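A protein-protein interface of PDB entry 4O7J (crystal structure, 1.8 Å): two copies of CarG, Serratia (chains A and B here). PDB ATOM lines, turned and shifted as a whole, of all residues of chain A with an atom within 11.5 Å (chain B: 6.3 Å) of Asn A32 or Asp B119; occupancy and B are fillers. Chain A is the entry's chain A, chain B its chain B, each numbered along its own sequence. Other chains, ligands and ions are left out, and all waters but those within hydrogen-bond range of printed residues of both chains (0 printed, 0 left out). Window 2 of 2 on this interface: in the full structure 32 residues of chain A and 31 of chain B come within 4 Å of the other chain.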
ATOM      1  N   GLN A  28      14.295  16.987  19.185  1.00  0.00           N
ATOM      2  CA  GLN A  28      14.811  18.173  18.575  1.00  0.00           C
ATOM      3  C   GLN A  28      14.234  19.385  19.194  1.00  0.00           C
ATOM      4  O   GLN A  28      13.171  19.335  19.679  1.00  0.00           O
ATOM      5  CB  GLN A  28      14.460  18.155  17.139  1.00  0.00           C
ATOM      6  CG  GLN A  28      13.003  17.970  16.887  1.00  0.00           C
ATOM      7  CD  GLN A  28      12.710  17.355  15.508  1.00  0.00           C
ATOM      8  OE1 GLN A  28      12.815  16.161  15.330  1.00  0.00           O
ATOM      9  NE2 GLN A  28      12.333  18.188  14.561  1.00  0.00           N
ATOM     10  N   PHE A  29      14.972  20.470  19.155  1.00  0.00           N
ATOM     11  CA  PHE A  29      14.466  21.760  19.582  1.00  0.00           C
ATOM     12  C   PHE A  29      13.911  22.404  18.336  1.00  0.00           C
ATOM     13  O   PHE A  29      14.674  22.806  17.456  1.00  0.00           O
ATOM     14  CB  PHE A  29      15.542  22.621  20.197  1.00  0.00           C
ATOM     15  CG  PHE A  29      15.086  24.007  20.564  1.00  0.00           C
ATOM     16  CD1 PHE A  29      13.873  24.188  21.187  1.00  0.00           C
ATOM     17  CD2 PHE A  29      15.870  25.119  20.284  1.00  0.00           C
ATOM     18  CE1 PHE A  29      13.438  25.457  21.545  1.00  0.00           C
ATOM     19  CE2 PHE A  29      15.464  26.389  20.646  1.00  0.00           C
ATOM     20  CZ  PHE A  29      14.237  26.562  21.257  1.00  0.00           C
ATOM     21  N   ASP A  30      12.602  22.570  18.341  1.00  0.00           N
ATOM     22  CA  ASP A  30      11.851  23.236  17.293  1.00  0.00           C
ATOM     23  C   ASP A  30      11.662  24.701  17.645  1.00  0.00           C
ATOM     24  O   ASP A  30      10.851  25.007  18.447  1.00  0.00           O
ATOM     25  CB  ASP A  30      10.485  22.573  17.177  1.00  0.00           C
ATOM     26  CG  ASP A  30      10.551  21.244  16.567  1.00  0.00           C
ATOM     27  OD1 ASP A  30      11.270  21.092  15.608  1.00  0.00           O
ATOM     28  OD2 ASP A  30       9.890  20.332  17.010  1.00  0.00           O
ATOM     29  N   ASN A  31      12.474  25.573  17.111  1.00  0.00           N
ATOM     30  CA  ASN A  31      12.158  26.991  17.186  1.00  0.00           C
ATOM     31  C   ASN A  31      11.938  27.590  15.818  1.00  0.00           C
ATOM     32  O   ASN A  31      12.193  28.731  15.598  1.00  0.00           O
ATOM     33  CB  ASN A  31      13.122  27.796  18.070  1.00  0.00           C
ATOM     34  CG  ASN A  31      14.484  27.908  17.486  1.00  0.00           C
ATOM     35  OD1 ASN A  31      14.855  27.126  16.650  1.00  0.00           O
ATOM     36  ND2 ASN A  31      15.220  28.915  17.903  1.00  0.00           N
ATOM     37  N   ASN A  32      11.417  26.755  14.936  1.00  0.00           N
ATOM     38  CA  ASN A  32      10.769  27.115  13.687  1.00  0.00           C
ATOM     39  C   ASN A  32      11.824  27.441  12.624  1.00  0.00           C
ATOM     40  O   ASN A  32      11.872  28.528  12.129  1.00  0.00           O
ATOM     41  CB  ASN A  32       9.733  28.242  13.885  1.00  0.00           C
ATOM     42  CG  ASN A  32       8.406  27.745  14.479  1.00  0.00           C
ATOM     43  OD1 ASN A  32       7.833  26.787  14.016  1.00  0.00           O
ATOM     44  ND2 ASN A  32       7.931  28.422  15.490  1.00  0.00           N
ATOM     45  N   THR A  33      12.679  26.475  12.312  1.00  0.00           N
ATOM     46  CA  THR A  33      13.681  26.608  11.257  1.00  0.00           C
ATOM     47  C   THR A  33      13.608  25.356  10.379  1.00  0.00           C
ATOM     48  O   THR A  33      12.928  24.437  10.747  1.00  0.00           O
ATOM     49  CB  THR A  33      15.102  26.800  11.833  1.00  0.00           C
ATOM     50  OG1 THR A  33      15.561  25.568  12.373  1.00  0.00           O
ATOM     51  CG2 THR A  33      15.150  27.845  12.934  1.00  0.00           C
ATOM     52  N   SER A  34      14.271  25.308   9.226  1.00  0.00           N
ATOM     53  CA  SER A  34      14.194  24.120   8.362  1.00  0.00           C
ATOM     54  C   SER A  34      14.858  22.862   8.917  1.00  0.00           C
ATOM     55  O   SER A  34      14.411  21.718   8.645  1.00  0.00           O
ATOM     56  CB  SER A  34      14.725  24.412   6.966  1.00  0.00           C
ATOM     57  OG  SER A  34      16.064  24.857   7.021  1.00  0.00           O
ATOM     58  N   HIS A  35      15.893  23.083   9.716  1.00  0.00           N
ATOM     59  CA  HIS A  35      16.714  22.013  10.237  1.00  0.00           C
ATOM     60  C   HIS A  35      16.779  22.270  11.725  1.00  0.00           C
ATOM     61  O   HIS A  35      17.617  23.028  12.201  1.00  0.00           O
ATOM     62  CB  HIS A  35      18.079  22.062   9.574  1.00  0.00           C
ATOM     63  CG  HIS A  35      18.020  22.202   8.087  1.00  0.00           C
ATOM     64  ND1 HIS A  35      17.707  21.149   7.255  1.00  0.00           N
ATOM     65  CD2 HIS A  35      18.265  23.262   7.281  1.00  0.00           C
ATOM     66  CE1 HIS A  35      17.721  21.561   6.001  1.00  0.00           C
ATOM     67  NE2 HIS A  35      18.048  22.843   5.990  1.00  0.00           N
ATOM     68  N   PRO A  36      15.790  21.751  12.451  1.00  0.00           N
ATOM     69  CA  PRO A  36      15.858  21.800  13.912  1.00  0.00           C
ATOM     70  C   PRO A  36      17.083  21.065  14.424  1.00  0.00           C
ATOM     71  O   PRO A  36      17.511  20.057  13.847  1.00  0.00           O
ATOM     72  CB  PRO A  36      14.563  21.145  14.381  1.00  0.00           C
ATOM     73  CG  PRO A  36      13.852  20.658  13.159  1.00  0.00           C
ATOM     74  CD  PRO A  36      14.658  20.965  11.937  1.00  0.00           C
ATOM     75  N   ASN A  37      17.607  21.534  15.549  1.00  0.00           N
ATOM     76  CA  ASN A  37      18.762  20.921  16.157  1.00  0.00           C
ATOM     77  C   ASN A  37      18.336  19.720  16.991  1.00  0.00           C
ATOM     78  O   ASN A  37      17.532  19.864  17.890  1.00  0.00           O
ATOM     79  CB  ASN A  37      19.509  21.953  17.026  1.00  0.00           C
ATOM     80  CG  ASN A  37      20.373  22.896  16.176  1.00  0.00           C
ATOM     81  OD1 ASN A  37      20.520  24.081  16.492  1.00  0.00           O
ATOM     82  ND2 ASN A  37      20.955  22.361  15.094  1.00  0.00           N
ATOM     83  N   LEU A  38      18.877  18.569  16.667  1.00  0.00           N
ATOM     84  CA  LEU A  38      18.689  17.340  17.438  1.00  0.00           C
ATOM     85  C   LEU A  38      19.522  17.391  18.687  1.00  0.00           C
ATOM     86  O   LEU A  38      20.652  17.827  18.685  1.00  0.00           O
ATOM     87  CB  LEU A  38      19.078  16.106  16.643  1.00  0.00           C
ATOM     88  CG  LEU A  38      18.236  15.745  15.439  1.00  0.00           C
ATOM     89  CD1 LEU A  38      18.686  14.389  14.886  1.00  0.00           C
ATOM     90  CD2 LEU A  38      16.783  15.665  15.825  1.00  0.00           C
ATOM     91  N   ARG A  68      24.153  24.183  13.947  1.00  0.00           N
ATOM     92  CA  ARG A  68      24.172  24.572  12.545  1.00  0.00           C
ATOM     93  C   ARG A  68      24.338  26.035  12.480  1.00  0.00           C
ATOM     94  O   ARG A  68      23.806  26.776  13.329  1.00  0.00           O
ATOM     95  CB  ARG A  68      22.878  24.263  11.844  1.00  0.00           C
ATOM     96  CG  ARG A  68      22.498  22.850  12.077  1.00  0.00           C
ATOM     97  CD  ARG A  68      21.131  22.518  11.561  1.00  0.00           C
ATOM     98  NE  ARG A  68      21.348  21.968  10.265  1.00  0.00           N
ATOM     99  CZ  ARG A  68      21.245  20.700   9.900  1.00  0.00           C
ATOM    100  NH1 ARG A  68      20.852  19.745  10.726  1.00  0.00           N
ATOM    101  NH2 ARG A  68      21.520  20.409   8.631  1.00  0.00           N
ATOM    102  N   SER A  70      23.530  28.635  10.640  1.00  0.00           N
ATOM    103  CA  SER A  70      22.440  29.580  10.658  1.00  0.00           C
ATOM    104  C   SER A  70      21.234  28.746  10.354  1.00  0.00           C
ATOM    105  O   SER A  70      21.322  27.514  10.284  1.00  0.00           O
ATOM    106  CB  SER A  70      22.600  30.622   9.550  1.00  0.00           C
ATOM    107  OG  SER A  70      22.237  30.063   8.294  1.00  0.00           O
ATOM    108  N   ALA A  71      20.112  29.394  10.095  1.00  0.00           N
ATOM    109  CA  ALA A  71      18.919  28.644   9.797  1.00  0.00           C
ATOM    110  C   ALA A  71      19.083  27.739   8.543  1.00  0.00           C
ATOM    111  O   ALA A  71      18.492  26.626   8.515  1.00  0.00           O
ATOM    112  CB  ALA A  71      17.726  29.597   9.675  1.00  0.00           C
ATOM    113  N   SER A  72      19.987  28.148   7.622  1.00  0.00           N
ATOM    114  CA  SER A  72      19.847  27.956   6.161  1.00  0.00           C
ATOM    115  C   SER A  72      20.460  26.688   5.499  1.00  0.00           C
ATOM    116  O   SER A  72      19.735  25.795   5.042  1.00  0.00           O
ATOM    117  CB  SER A  72      20.391  29.211   5.457  1.00  0.00           C
ATOM    118  OG  SER A  72      20.307  29.101   4.045  1.00  0.00           O
ATOM    119  N   SER B 117       3.391  27.924  18.908  1.00  0.00           N
ATOM    120  CA  SER B 117       3.673  29.162  18.135  1.00  0.00           C
ATOM    121  C   SER B 117       4.163  28.657  16.780  1.00  0.00           C
ATOM    122  O   SER B 117       5.306  28.334  16.615  1.00  0.00           O
ATOM    123  CB  SER B 117       4.695  30.064  18.829  1.00  0.00           C
ATOM    124  OG  SER B 117       4.286  30.514  20.132  1.00  0.00           O
ATOM    125  N   ARG B 118       3.233  28.468  15.838  1.00  0.00           N
ATOM    126  CA  ARG B 118       3.537  27.667  14.645  1.00  0.00           C
ATOM    127  C   ARG B 118       4.152  28.532  13.571  1.00  0.00           C
ATOM    128  O   ARG B 118       3.676  29.594  13.363  1.00  0.00           O
ATOM    129  CB  ARG B 118       2.275  26.993  14.104  1.00  0.00           C
ATOM    130  CG  ARG B 118       2.555  25.824  13.151  1.00  0.00           C
ATOM    131  CD  ARG B 118       2.160  24.495  13.746  1.00  0.00           C
ATOM    132  NE  ARG B 118       3.163  23.462  13.431  1.00  0.00           N
ATOM    133  CZ  ARG B 118       3.263  22.299  14.074  1.00  0.00           C
ATOM    134  NH1 ARG B 118       2.410  21.981  15.054  1.00  0.00           N
ATOM    135  NH2 ARG B 118       4.219  21.440  13.733  1.00  0.00           N
ATOM    136  N   ASP B 119       5.223  28.059  12.924  1.00  0.00           N
ATOM    137  CA  ASP B 119       5.918  28.767  11.810  1.00  0.00           C
ATOM    138  C   ASP B 119       6.313  30.234  12.131  1.00  0.00           C
ATOM    139  O   ASP B 119       6.394  31.092  11.230  1.00  0.00           O
ATOM    140  CB  ASP B 119       5.092  28.656  10.499  1.00  0.00           C
ATOM    141  N   ASP B 120       6.572  30.502  13.415  1.00  0.00           N
ATOM    142  CA  ASP B 120       6.816  31.852  13.934  1.00  0.00           C
ATOM    143  C   ASP B 120       8.321  32.028  14.165  1.00  0.00           C
ATOM    144  O   ASP B 120       8.956  31.156  14.761  1.00  0.00           O
ATOM    145  CB  ASP B 120       6.035  32.021  15.256  1.00  0.00           C
ATOM    146  CG  ASP B 120       5.347  33.363  15.383  1.00  0.00           C
ATOM    147  OD1 ASP B 120       4.116  33.439  15.124  1.00  0.00           O
ATOM    148  OD2 ASP B 120       6.031  34.335  15.784  1.00  0.00           O
ATOM    149  N   PRO B 121       8.908  33.161  13.693  1.00  0.00           N
ATOM    150  CA  PRO B 121      10.365  33.188  13.451  1.00  0.00           C
ATOM    151  C   PRO B 121      11.277  33.080  14.665  1.00  0.00           C
ATOM    152  O   PRO B 121      11.299  33.977  15.517  1.00  0.00           O
ATOM    153  CB  PRO B 121      10.601  34.533  12.714  1.00  0.00           C
ATOM    154  CG  PRO B 121       9.386  35.367  12.979  1.00  0.00           C
ATOM    155  CD  PRO B 121       8.252  34.419  13.285  1.00  0.00           C
ATOM    156  N   GLY B 122      12.029  31.984  14.736  1.00  0.00           N
ATOM    157  CA  GLY B 122      12.953  31.801  15.836  1.00  0.00           C
ATOM    158  C   GLY B 122      12.276  31.676  17.197  1.00  0.00           C
ATOM    159  O   GLY B 122      12.966  31.728  18.175  1.00  0.00           O
ATOM    160  N   VAL B 123      10.939  31.541  17.267  1.00  0.00           N
ATOM    161  CA  VAL B 123      10.211  31.406  18.558  1.00  0.00           C
ATOM    162  C   VAL B 123       9.990  29.881  18.804  1.00  0.00           C
ATOM    163  O   VAL B 123       9.714  29.126  17.868  1.00  0.00           O
ATOM    164  CB  VAL B 123       8.872  32.170  18.491  1.00  0.00           C
ATOM    165  CG1 VAL B 123       7.989  31.948  19.717  1.00  0.00           C
ATOM    166  CG2 VAL B 123       9.134  33.662  18.293  1.00  0.00           C
ATOM    167  N   PRO B 124      10.112  29.415  20.059  1.00  0.00           N
ATOM    168  CA  PRO B 124       9.874  27.963  20.268  1.00  0.00           C
ATOM    169  C   PRO B 124       8.480  27.570  19.810  1.00  0.00           C
ATOM    170  O   PRO B 124       7.498  28.247  20.125  1.00  0.00           O
ATOM    171  CB  PRO B 124      10.015  27.795  21.774  1.00  0.00           C
ATOM    172  CG  PRO B 124      10.813  28.990  22.212  1.00  0.00           C
ATOM    173  CD  PRO B 124      10.425  30.115  21.315  1.00  0.00           C
ATOM    174  N   LEU B 125       8.420  26.483  19.032  1.00  0.00           N
ATOM    175  CA  LEU B 125       7.185  25.952  18.550  1.00  0.00           C
ATOM    176  C   LEU B 125       6.280  25.563  19.728  1.00  0.00           C
ATOM    177  O   LEU B 125       5.059  25.881  19.736  1.00  0.00           O
ATOM    178  CB  LEU B 125       7.452  24.718  17.723  1.00  0.00           C
ATOM    179  CG  LEU B 125       6.232  23.974  17.227  1.00  0.00           C
ATOM    180  CD1 LEU B 125       5.324  24.918  16.464  1.00  0.00           C
ATOM    181  CD2 LEU B 125       6.693  22.808  16.390  1.00  0.00           C
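N of Asp B119 is in hydrogen-bond range of OD1 of Asn A32 (3.1 Å).
The backbone NH of Gly B122 lies close to the backbone carbonyl oxygen of Asn A31, 3.4 Å away.
The backbone carbonyl oxygen of Asp B120 sits at hydrogen-bond distance from the side-chain amide nitrogen of Asn A32, at 3.0 Å.
O of Asp A30 lies within hydrogen-bond range of N of Leu B125 (2.9 Å).
The backbone carbonyl oxygen (O) of Val B123 sits close to the backbone carbonyl oxygen (O) of Asn A31, at 3.4 Å.
The side-chain amide nitrogen (ND2) of Asn A32 is in hydrogen-bond range of the backbone carbonyl oxygen (O) of Ser B117, at 2.9 Å.
O of Val B123 is in hydrogen-bond range of ND2 of Asn A32 (3.1 Å).
The side-chain amide nitrogen of Gln A28 is in hydrogen-bond range of the side-chain carboxylate of Asp A30 (3.3 Å).
The backbone NH of Ser B117 sits at hydrogen-bond distance from the backbone carbonyl oxygen of Leu B125 (2.8 Å).
Asp A30 touches Pro B124 (O to CA, 3.6 Å).
Pro B124 touches Asn A31 (CA to CB, 3.9 Å).
Leu B125 touches Asn A32 (CD1 to OD1, 3.97 Å).
Of the printed residues of chain B, Asp A30 touches Pro B124 and Leu B125.
Of the printed residues of chain B, Asn A31 touches Gly B122, Val B123 and Pro B124.
Asn A32 touches just these residues of chain B: Ser B117 (2.9 Å), Asp B119 (3.1 Å), Asp B120 (3.0 Å), Val B123 (3.1 Å) and Leu B125 (3.97 Å).
Of chain A, only Asn A32 (2.9 Å) comes within 4 Å of Ser B117.
No residue of chain A comes within 4 Å of Arg B118.
Asp B119 touches one residue of chain A.
Asp B120 touches one residue of chain A.
Of chain A, only Asn A31 (3.2 Å) comes within 4 Å of Gly B122.
Of chain A, only Asn A31 (3.3 Å) and Asn A32 (3.1 Å) come within 4 Å of Val B123.
Pro B124 touches just these residues of chain A: Asp A30 and Asn A31.
Leu B125 touches two residues of chain A.
Of the 15 printed residues of chain A, 3 touch a printed residue of chain B.
Hydrophobic or aromatic side chains of chain B within 4 Å of the printed part of chain A: Leu B125.
Among the printed residues, 10 pairs touch across the chains.
Among the printed residues, no Asp or Glu carboxylate lies within 4 Å of a Lys or Arg side-chain nitrogen of the other chain.
No position is printed for both chains.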
